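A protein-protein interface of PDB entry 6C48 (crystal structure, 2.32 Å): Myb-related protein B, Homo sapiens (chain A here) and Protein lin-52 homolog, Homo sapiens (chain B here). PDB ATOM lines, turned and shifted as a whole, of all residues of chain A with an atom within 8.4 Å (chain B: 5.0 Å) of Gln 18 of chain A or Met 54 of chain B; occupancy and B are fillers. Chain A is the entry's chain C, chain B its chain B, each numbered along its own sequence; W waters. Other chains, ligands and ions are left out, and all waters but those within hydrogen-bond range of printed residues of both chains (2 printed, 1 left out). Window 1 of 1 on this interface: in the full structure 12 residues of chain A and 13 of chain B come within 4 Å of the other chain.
The backbone carbonyl oxygen (O) of Ser 51 of chain B is in hydrogen-bond range of the side-chain hydroxyl (OG1) of Thr 55 of chain B (3.3 Å). OD1 of Asp 17 of chain A lies within salt-bridge range of NE of Arg 16 of chain A (3.9 Å). The side-chain amide oxygen (OE1) of Gln 18 of chain A lies close to the backbone carbonyl oxygen (O) of Gly 13 of chain A, 3.4 Å away.
Printed residues of chain A that touch a printed residue of chain B: Gly 13, Thr 15, Asp 17, Gln 18, Phe 20 and Met 21. Hydrophobic or aromatic side chains of chain A within 4 Å of the printed part of chain B: Phe 20 and Met 21. Among the printed residues, no Asp or Glu carboxylate lies within 4 Å of a Lys or Arg side-chain nitrogen of the other chain.
Of chain B, only Glu 50 and Met 54 come within 4 Å of Gln 18 of chain A. Met 54 of chain B touches just these residues of chain A: Gln 18 and Met 21. Of the printed residues of chain A, Thr 55 of chain B touches Asp 17. Of the printed residues of chain A, Lys 58 of chain B touches Asp 17 (3.4 Å), Phe 20 (3.5 Å) and Met 21 (3.6 Å). Of the printed residues of chain B, Met 21 of chain A touches Met 54 (3.6 Å), Gly 57 (3.5 Å) and Lys 58 (3.6 Å). Glu 23 of chain A touches none of the printed residues of chain B. The nearest residue of chain B that does not touch Gln 18 of chain A is Ser 51 of chain B (4.6 Å). The nearest printed residue of chain B that does not touch Gly 13 of chain A is Ser 51 of chain B (6.3 Å).
Among the printed residues, pairs that only touch across the chains: Gly 13 of chain A with Glu 50 of chain B (3.3 Å), Asp 17 of chain A with Lys 58 of chain B (3.4 Å), Met 21 of chain A with Gly 57 of chain B (3.5 Å), Phe 20 of chain A with Lys 58 of chain B (3.5 Å), Met 21 of chain A with Met 54 of chain B (3.6 Å), Thr 15 of chain A with Ser 51 of chain B (3.7 Å) and Gln 18 of chain A with Met 54 of chain B (3.8 Å).
Water W2 lies within hydrogen-bond range of OG1 of Thr 15 of chain A (2.7 Å), OG1 of Thr 55 of chain B (3.0 Å) and O of Ser 51 of chain B (3.1 Å). Water W1 bridges O of Gly 57 of chain B (2.7 Å) and SD of Met 21 of chain A (3.7 Å).
The side-chain carboxylate (OD2) of Asp 17 of chain A is in hydrogen-bond range of the side-chain hydroxyl (OG1) of Thr 55 of chain B (2.8 Å). SD of Met 21 of chain A lies close to N of Lys 58 of chain B (3.8 Å). The side-chain amide nitrogen (NE2) of Gln 18 of chain A sits at hydrogen-bond distance from the side-chain carboxylate (OE2) of Glu 50 of chain B (2.9 Å).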
ATOM      1  N   THR A   9      25.027  11.929  -2.015  1.00  0.00           N
ATOM      2  CA  THR A   9      23.848  11.605  -2.809  1.00  0.00           C
ATOM      3  C   THR A   9      22.800  11.076  -1.847  1.00  0.00           C
ATOM      4  O   THR A   9      21.645  11.501  -1.861  1.00  0.00           O
ATOM      5  CB  THR A   9      24.154  10.536  -3.873  1.00  0.00           C
ATOM      6  OG1 THR A   9      24.707  11.162  -5.038  1.00  0.00           O
ATOM      7  CG2 THR A   9      22.885   9.791  -4.260  1.00  0.00           C
ATOM      8  N   VAL A  10      23.225  10.140  -1.007  1.00  0.00           N
ATOM      9  CA  VAL A  10      22.367   9.572   0.021  1.00  0.00           C
ATOM     10  C   VAL A  10      22.059  10.615   1.091  1.00  0.00           C
ATOM     11  O   VAL A  10      20.896  10.931   1.354  1.00  0.00           O
ATOM     12  CB  VAL A  10      23.044   8.330   0.629  1.00  0.00           C
ATOM     13  CG1 VAL A  10      22.348   7.923   1.922  1.00  0.00           C
ATOM     14  CG2 VAL A  10      23.063   7.190  -0.367  1.00  0.00           C
ATOM     15  N   ALA A  11      23.096  11.210   1.678  1.00  0.00           N
ATOM     16  CA  ALA A  11      22.890  12.103   2.811  1.00  0.00           C
ATOM     17  C   ALA A  11      21.994  13.287   2.461  1.00  0.00           C
ATOM     18  O   ALA A  11      21.208  13.729   3.309  1.00  0.00           O
ATOM     19  CB  ALA A  11      24.238  12.596   3.336  1.00  0.00           C
ATOM     20  N   CYS A  12      22.036  13.773   1.218  1.00  0.00           N
ATOM     21  CA  CYS A  12      21.247  14.944   0.846  1.00  0.00           C
ATOM     22  C   CYS A  12      20.144  14.615  -0.153  1.00  0.00           C
ATOM     23  O   CYS A  12      19.746  15.473  -0.944  1.00  0.00           O
ATOM     24  CB  CYS A  12      22.134  16.057   0.281  1.00  0.00           C
ATOM     25  SG  CYS A  12      23.451  16.636   1.364  1.00  0.00           S
ATOM     26  N   GLY A  13      19.602  13.400  -0.090  1.00  0.00           N
ATOM     27  CA  GLY A  13      18.409  13.089  -0.845  1.00  0.00           C
ATOM     28  C   GLY A  13      18.510  13.349  -2.333  1.00  0.00           C
ATOM     29  O   GLY A  13      17.635  13.994  -2.913  1.00  0.00           O
ATOM     30  N   GLY A  14      19.579  12.866  -2.963  1.00  0.00           N
ATOM     31  CA  GLY A  14      19.782  13.062  -4.384  1.00  0.00           C
ATOM     32  C   GLY A  14      19.598  11.850  -5.272  1.00  0.00           C
ATOM     33  O   GLY A  14      19.990  11.903  -6.438  1.00  0.00           O
ATOM     34  N   THR A  15      19.038  10.748  -4.769  1.00  0.00           N
ATOM     35  CA  THR A  15      18.879   9.563  -5.608  1.00  0.00           C
ATOM     36  C   THR A  15      17.821   9.773  -6.687  1.00  0.00           C
ATOM     37  O   THR A  15      16.940  10.628  -6.577  1.00  0.00           O
ATOM     38  CB  THR A  15      18.500   8.342  -4.781  1.00  0.00           C
ATOM     39  OG1 THR A  15      17.201   8.538  -4.207  1.00  0.00           O
ATOM     40  CG2 THR A  15      19.539   8.136  -3.691  1.00  0.00           C
ATOM     41  N   ARG A  16      17.917   8.938  -7.730  1.00  0.00           N
ATOM     42  CA  ARG A  16      17.127   9.108  -8.953  1.00  0.00           C
ATOM     43  C   ARG A  16      15.622   9.094  -8.677  1.00  0.00           C
ATOM     44  O   ARG A  16      14.876   9.898  -9.250  1.00  0.00           O
ATOM     45  CB  ARG A  16      17.528   8.020  -9.961  1.00  0.00           C
ATOM     46  CG  ARG A  16      16.438   7.527 -10.874  1.00  0.00           C
ATOM     47  CD  ARG A  16      16.814   6.211 -11.601  1.00  0.00           C
ATOM     48  NE  ARG A  16      15.613   5.577 -12.158  1.00  0.00           N
ATOM     49  CZ  ARG A  16      15.599   4.538 -12.991  1.00  0.00           C
ATOM     50  NH1 ARG A  16      16.733   3.977 -13.390  1.00  0.00           N
ATOM     51  NH2 ARG A  16      14.434   4.055 -13.428  1.00  0.00           N
ATOM     52  N   ASP A  17      15.149   8.200  -7.800  1.00  0.00           N
ATOM     53  CA  ASP A  17      13.714   8.180  -7.511  1.00  0.00           C
ATOM     54  C   ASP A  17      13.276   9.386  -6.685  1.00  0.00           C
ATOM     55  O   ASP A  17      12.132   9.836  -6.820  1.00  0.00           O
ATOM     56  CB  ASP A  17      13.324   6.898  -6.784  1.00  0.00           C
ATOM     57  CG  ASP A  17      13.474   5.668  -7.648  1.00  0.00           C
ATOM     58  OD1 ASP A  17      13.418   5.790  -8.897  1.00  0.00           O
ATOM     59  OD2 ASP A  17      13.677   4.585  -7.062  1.00  0.00           O
ATOM     60  N   GLN A  18      14.152   9.920  -5.824  1.00  0.00           N
ATOM     61  CA  GLN A  18      13.766  11.099  -5.054  1.00  0.00           C
ATOM     62  C   GLN A  18      13.609  12.312  -5.958  1.00  0.00           C
ATOM     63  O   GLN A  18      12.638  13.065  -5.821  1.00  0.00           O
ATOM     64  CB  GLN A  18      14.776  11.401  -3.947  1.00  0.00           C
ATOM     65  CG  GLN A  18      14.477  12.688  -3.166  1.00  0.00           C
ATOM     66  CD  GLN A  18      14.909  12.608  -1.709  1.00  0.00           C
ATOM     67  OE1 GLN A  18      15.662  11.713  -1.317  1.00  0.00           O
ATOM     68  NE2 GLN A  18      14.429  13.535  -0.901  1.00  0.00           N
ATOM     69  N   LEU A  19      14.546  12.506  -6.897  1.00  0.00           N
ATOM     70  CA  LEU A  19      14.411  13.592  -7.868  1.00  0.00           C
ATOM     71  C   LEU A  19      13.156  13.402  -8.712  1.00  0.00           C
ATOM     72  O   LEU A  19      12.475  14.374  -9.062  1.00  0.00           O
ATOM     73  CB  LEU A  19      15.655  13.671  -8.757  1.00  0.00           C
ATOM     74  CG  LEU A  19      17.024  13.929  -8.089  1.00  0.00           C
ATOM     75  CD1 LEU A  19      18.189  13.798  -9.098  1.00  0.00           C
ATOM     76  CD2 LEU A  19      17.077  15.279  -7.387  1.00  0.00           C
ATOM     77  N   PHE A  20      12.822  12.151  -9.023  1.00  0.00           N
ATOM     78  CA  PHE A  20      11.587  11.862  -9.734  1.00  0.00           C
ATOM     79  C   PHE A  20      10.382  12.269  -8.901  1.00  0.00           C
ATOM     80  O   PHE A  20       9.504  13.001  -9.370  1.00  0.00           O
ATOM     81  CB  PHE A  20      11.541  10.375 -10.086  1.00  0.00           C
ATOM     82  CG  PHE A  20      10.271   9.942 -10.722  1.00  0.00           C
ATOM     83  CD1 PHE A  20       9.223   9.477  -9.955  1.00  0.00           C
ATOM     84  CD2 PHE A  20      10.124   9.989 -12.097  1.00  0.00           C
ATOM     85  CE1 PHE A  20       8.029   9.083 -10.546  1.00  0.00           C
ATOM     86  CE2 PHE A  20       8.935   9.587 -12.701  1.00  0.00           C
ATOM     87  CZ  PHE A  20       7.890   9.141 -11.920  1.00  0.00           C
ATOM     88  N   MET A  21      10.327  11.817  -7.655  1.00  0.00           N
ATOM     89  CA  MET A  21       9.205  12.135  -6.773  1.00  0.00           C
ATOM     90  C   MET A  21       9.043  13.635  -6.542  1.00  0.00           C
ATOM     91  O   MET A  21       7.928  14.118  -6.394  1.00  0.00           O
ATOM     92  CB  MET A  21       9.369  11.416  -5.437  1.00  0.00           C
ATOM     93  CG  MET A  21       9.141   9.927  -5.566  1.00  0.00           C
ATOM     94  SD  MET A  21       7.352   9.520  -6.286  1.00  0.00           S
ATOM     95  CE  MET A  21       6.360   9.341  -4.614  1.00  0.00           C
ATOM     96  N   GLN A  22      10.160  14.363  -6.524  1.00  0.00           N
ATOM     97  CA  GLN A  22      10.096  15.813  -6.361  1.00  0.00           C
ATOM     98  C   GLN A  22       9.446  16.453  -7.573  1.00  0.00           C
ATOM     99  O   GLN A  22       8.683  17.414  -7.439  1.00  0.00           O
ATOM    100  CB  GLN A  22      11.496  16.384  -6.125  1.00  0.00           C
ATOM    101  CG  GLN A  22      12.059  16.007  -4.767  1.00  0.00           C
ATOM    102  CD  GLN A  22      13.526  16.393  -4.562  1.00  0.00           C
ATOM    103  OE1 GLN A  22      14.244  16.759  -5.502  1.00  0.00           O
ATOM    104  NE2 GLN A  22      13.975  16.296  -3.319  1.00  0.00           N
ATOM    105  N   GLU A  23       9.739  15.918  -8.759  1.00  0.00           N
ATOM    106  CA  GLU A  23       9.116  16.375  -9.997  1.00  0.00           C
ATOM    107  C   GLU A  23       7.608  16.115  -9.988  1.00  0.00           C
ATOM    108  O   GLU A  23       6.813  16.999 -10.323  1.00  0.00           O
ATOM    109  CB  GLU A  23       9.799  15.661 -11.174  1.00  0.00           C
ATOM    110  CG  GLU A  23       9.256  15.933 -12.566  1.00  0.00           C
ATOM    111  CD  GLU A  23       9.057  14.619 -13.372  1.00  0.00           C
ATOM    112  OE1 GLU A  23       8.418  14.667 -14.465  1.00  0.00           O
ATOM    113  OE2 GLU A  23       9.539  13.538 -12.909  1.00  0.00           O
ATOM    114  N   LYS A  24       7.192  14.914  -9.578  1.00  0.00           N
ATOM    115  CA  LYS A  24       5.765  14.611  -9.484  1.00  0.00           C
ATOM    116  C   LYS A  24       5.078  15.492  -8.446  1.00  0.00           C
ATOM    117  O   LYS A  24       3.929  15.914  -8.637  1.00  0.00           O
ATOM    118  CB  LYS A  24       5.571  13.140  -9.129  1.00  0.00           C
ATOM    119  CG  LYS A  24       6.027  12.162 -10.169  1.00  0.00           C
ATOM    120  CD  LYS A  24       5.081  12.113 -11.359  1.00  0.00           C
ATOM    121  CE  LYS A  24       5.866  12.042 -12.666  1.00  0.00           C
ATOM    122  NZ  LYS A  24       5.186  11.253 -13.736  1.00  0.00           N
ATOM    123  N   ALA A  25       5.761  15.777  -7.333  1.00  0.00           N
ATOM    124  CA  ALA A  25       5.155  16.612  -6.301  1.00  0.00           C
ATOM    125  C   ALA A  25       4.937  18.032  -6.805  1.00  0.00           C
ATOM    126  O   ALA A  25       3.868  18.615  -6.596  1.00  0.00           O
ATOM    127  CB  ALA A  25       6.021  16.608  -5.038  1.00  0.00           C
ATOM    128  N   ARG A  26       5.923  18.587  -7.510  1.00  0.00           N
ATOM    129  CA  ARG A  26       5.736  19.898  -8.127  1.00  0.00           C
ATOM    130  C   ARG A  26       4.542  19.892  -9.071  1.00  0.00           C
ATOM    131  O   ARG A  26       3.705  20.796  -9.033  1.00  0.00           O
ATOM    132  CB  ARG A  26       7.010  20.323  -8.862  1.00  0.00           C
ATOM    133  CG  ARG A  26       8.112  20.788  -7.919  1.00  0.00           C
ATOM    134  CD  ARG A  26       9.198  21.525  -8.663  1.00  0.00           C
ATOM    135  NE  ARG A  26       9.891  20.679  -9.632  1.00  0.00           N
ATOM    136  CZ  ARG A  26      10.919  19.892  -9.339  1.00  0.00           C
ATOM    137  NH1 ARG A  26      11.385  19.838  -8.094  1.00  0.00           N
ATOM    138  NH2 ARG A  26      11.488  19.174 -10.294  1.00  0.00           N
ATOM    139  N   GLU B  50      15.255   7.762   3.735  1.00  0.00           N
ATOM    140  CA  GLU B  50      14.554   8.650   2.822  1.00  0.00           C
ATOM    141  C   GLU B  50      14.528   8.087   1.400  1.00  0.00           C
ATOM    142  O   GLU B  50      13.473   8.035   0.760  1.00  0.00           O
ATOM    143  CB  GLU B  50      15.240  10.008   2.862  1.00  0.00           C
ATOM    144  CG  GLU B  50      14.605  11.116   2.075  1.00  0.00           C
ATOM    145  CD  GLU B  50      15.574  12.280   1.912  1.00  0.00           C
ATOM    146  OE1 GLU B  50      16.790  12.028   1.818  1.00  0.00           O
ATOM    147  OE2 GLU B  50      15.135  13.437   1.900  1.00  0.00           O
ATOM    148  N   SER B  51      15.681   7.654   0.889  1.00  0.00           N
ATOM    149  CA  SER B  51      15.709   7.154  -0.478  1.00  0.00           C
ATOM    150  C   SER B  51      14.872   5.888  -0.629  1.00  0.00           C
ATOM    151  O   SER B  51      14.210   5.703  -1.663  1.00  0.00           O
ATOM    152  CB  SER B  51      17.149   6.901  -0.918  1.00  0.00           C
ATOM    153  OG  SER B  51      17.735   5.877  -0.137  1.00  0.00           O
ATOM    154  N   ARG B  52      14.832   5.042   0.402  1.00  0.00           N
ATOM    155  CA  ARG B  52      14.029   3.830   0.299  1.00  0.00           C
ATOM    156  C   ARG B  52      12.543   4.155   0.202  1.00  0.00           C
ATOM    157  O   ARG B  52      11.830   3.553  -0.610  1.00  0.00           O
ATOM    158  CB  ARG B  52      14.290   2.907   1.477  1.00  0.00           C
ATOM    159  CG  ARG B  52      13.340   1.753   1.495  1.00  0.00           C
ATOM    160  CD  ARG B  52      13.201   1.235   2.884  1.00  0.00           C
ATOM    161  NE  ARG B  52      12.485  -0.030   2.910  1.00  0.00           N
ATOM    162  CZ  ARG B  52      11.238  -0.175   3.332  1.00  0.00           C
ATOM    163  NH1 ARG B  52      10.550   0.868   3.780  1.00  0.00           N
ATOM    164  NH2 ARG B  52      10.696  -1.374   3.328  1.00  0.00           N
ATOM    165  N   GLU B  53      12.068   5.121   0.991  1.00  0.00           N
ATOM    166  CA  GLU B  53      10.660   5.508   0.923  1.00  0.00           C
ATOM    167  C   GLU B  53      10.331   6.253  -0.363  1.00  0.00           C
ATOM    168  O   GLU B  53       9.177   6.239  -0.805  1.00  0.00           O
ATOM    169  CB  GLU B  53      10.265   6.366   2.125  1.00  0.00           C
ATOM    170  CG  GLU B  53      10.516   5.722   3.476  1.00  0.00           C
ATOM    171  CD  GLU B  53       9.831   4.378   3.655  1.00  0.00           C
ATOM    172  OE1 GLU B  53       8.690   4.190   3.183  1.00  0.00           O
ATOM    173  OE2 GLU B  53      10.436   3.510   4.300  1.00  0.00           O
ATOM    174  N   MET B  54      11.316   6.903  -0.984  1.00  0.00           N
ATOM    175  CA  MET B  54      11.060   7.534  -2.277  1.00  0.00           C
ATOM    176  C   MET B  54      10.897   6.486  -3.379  1.00  0.00           C
ATOM    177  O   MET B  54      10.062   6.648  -4.278  1.00  0.00           O
ATOM    178  CB  MET B  54      12.177   8.526  -2.600  1.00  0.00           C
ATOM    179  CG  MET B  54      12.153   9.792  -1.713  1.00  0.00           C
ATOM    180  SD  MET B  54      10.705  10.837  -2.068  1.00  0.00           S
ATOM    181  CE  MET B  54      10.898  12.103  -0.812  1.00  0.00           C
ATOM    182  N   THR B  55      11.698   5.413  -3.332  1.00  0.00           N
ATOM    183  CA  THR B  55      11.505   4.281  -4.233  1.00  0.00           C
ATOM    184  C   THR B  55      10.155   3.587  -3.996  1.00  0.00           C
ATOM    185  O   THR B  55       9.477   3.208  -4.951  1.00  0.00           O
ATOM    186  CB  THR B  55      12.654   3.291  -4.072  1.00  0.00           C
ATOM    187  OG1 THR B  55      13.888   3.940  -4.392  1.00  0.00           O
ATOM    188  CG2 THR B  55      12.455   2.087  -4.983  1.00  0.00           C
ATOM    189  N   ARG B  56       9.751   3.412  -2.729  1.00  0.00           N
ATOM    190  CA  ARG B  56       8.453   2.800  -2.430  1.00  0.00           C
ATOM    191  C   ARG B  56       7.313   3.625  -2.995  1.00  0.00           C
ATOM    192  O   ARG B  56       6.399   3.092  -3.630  1.00  0.00           O
ATOM    193  CB  ARG B  56       8.241   2.694  -0.926  1.00  0.00           C
ATOM    194  CG  ARG B  56       8.945   1.617  -0.205  1.00  0.00           C
ATOM    195  CD  ARG B  56       8.522   1.686   1.249  1.00  0.00           C
ATOM    196  NE  ARG B  56       7.184   1.164   1.460  1.00  0.00           N
ATOM    197  CZ  ARG B  56       6.514   1.282   2.605  1.00  0.00           C
ATOM    198  NH1 ARG B  56       7.053   1.922   3.637  1.00  0.00           N
ATOM    199  NH2 ARG B  56       5.309   0.755   2.724  1.00  0.00           N
ATOM    200  N   GLY B  57       7.345   4.939  -2.752  1.00  0.00           N
ATOM    201  CA  GLY B  57       6.246   5.794  -3.164  1.00  0.00           C
ATOM    202  C   GLY B  57       6.117   5.894  -4.666  1.00  0.00           C
ATOM    203  O   GLY B  57       5.004   6.017  -5.186  1.00  0.00           O
ATOM    204  N   LYS B  58       7.248   5.860  -5.382  1.00  0.00           N
ATOM    205  CA  LYS B  58       7.212   5.941  -6.839  1.00  0.00           C
ATOM    206  C   LYS B  58       6.424   4.777  -7.432  1.00  0.00           C
ATOM    207  O   LYS B  58       5.533   4.970  -8.266  1.00  0.00           O
ATOM    208  CB  LYS B  58       8.640   5.979  -7.389  1.00  0.00           C
ATOM    209  CG  LYS B  58       8.726   6.013  -8.908  1.00  0.00           C
ATOM    210  CD  LYS B  58      10.086   5.500  -9.372  1.00  0.00           C
ATOM    211  CE  LYS B  58      10.492   6.129 -10.689  1.00  0.00           C
ATOM    212  NZ  LYS B  58       9.721   5.573 -11.809  1.00  0.00           N
HETATM  213  O   HOH W   1       3.992   8.050  -6.706  1.00  0.00           O
HETATM  214  O   HOH W   2      15.809   6.217  -4.326  1.00  0.00           O
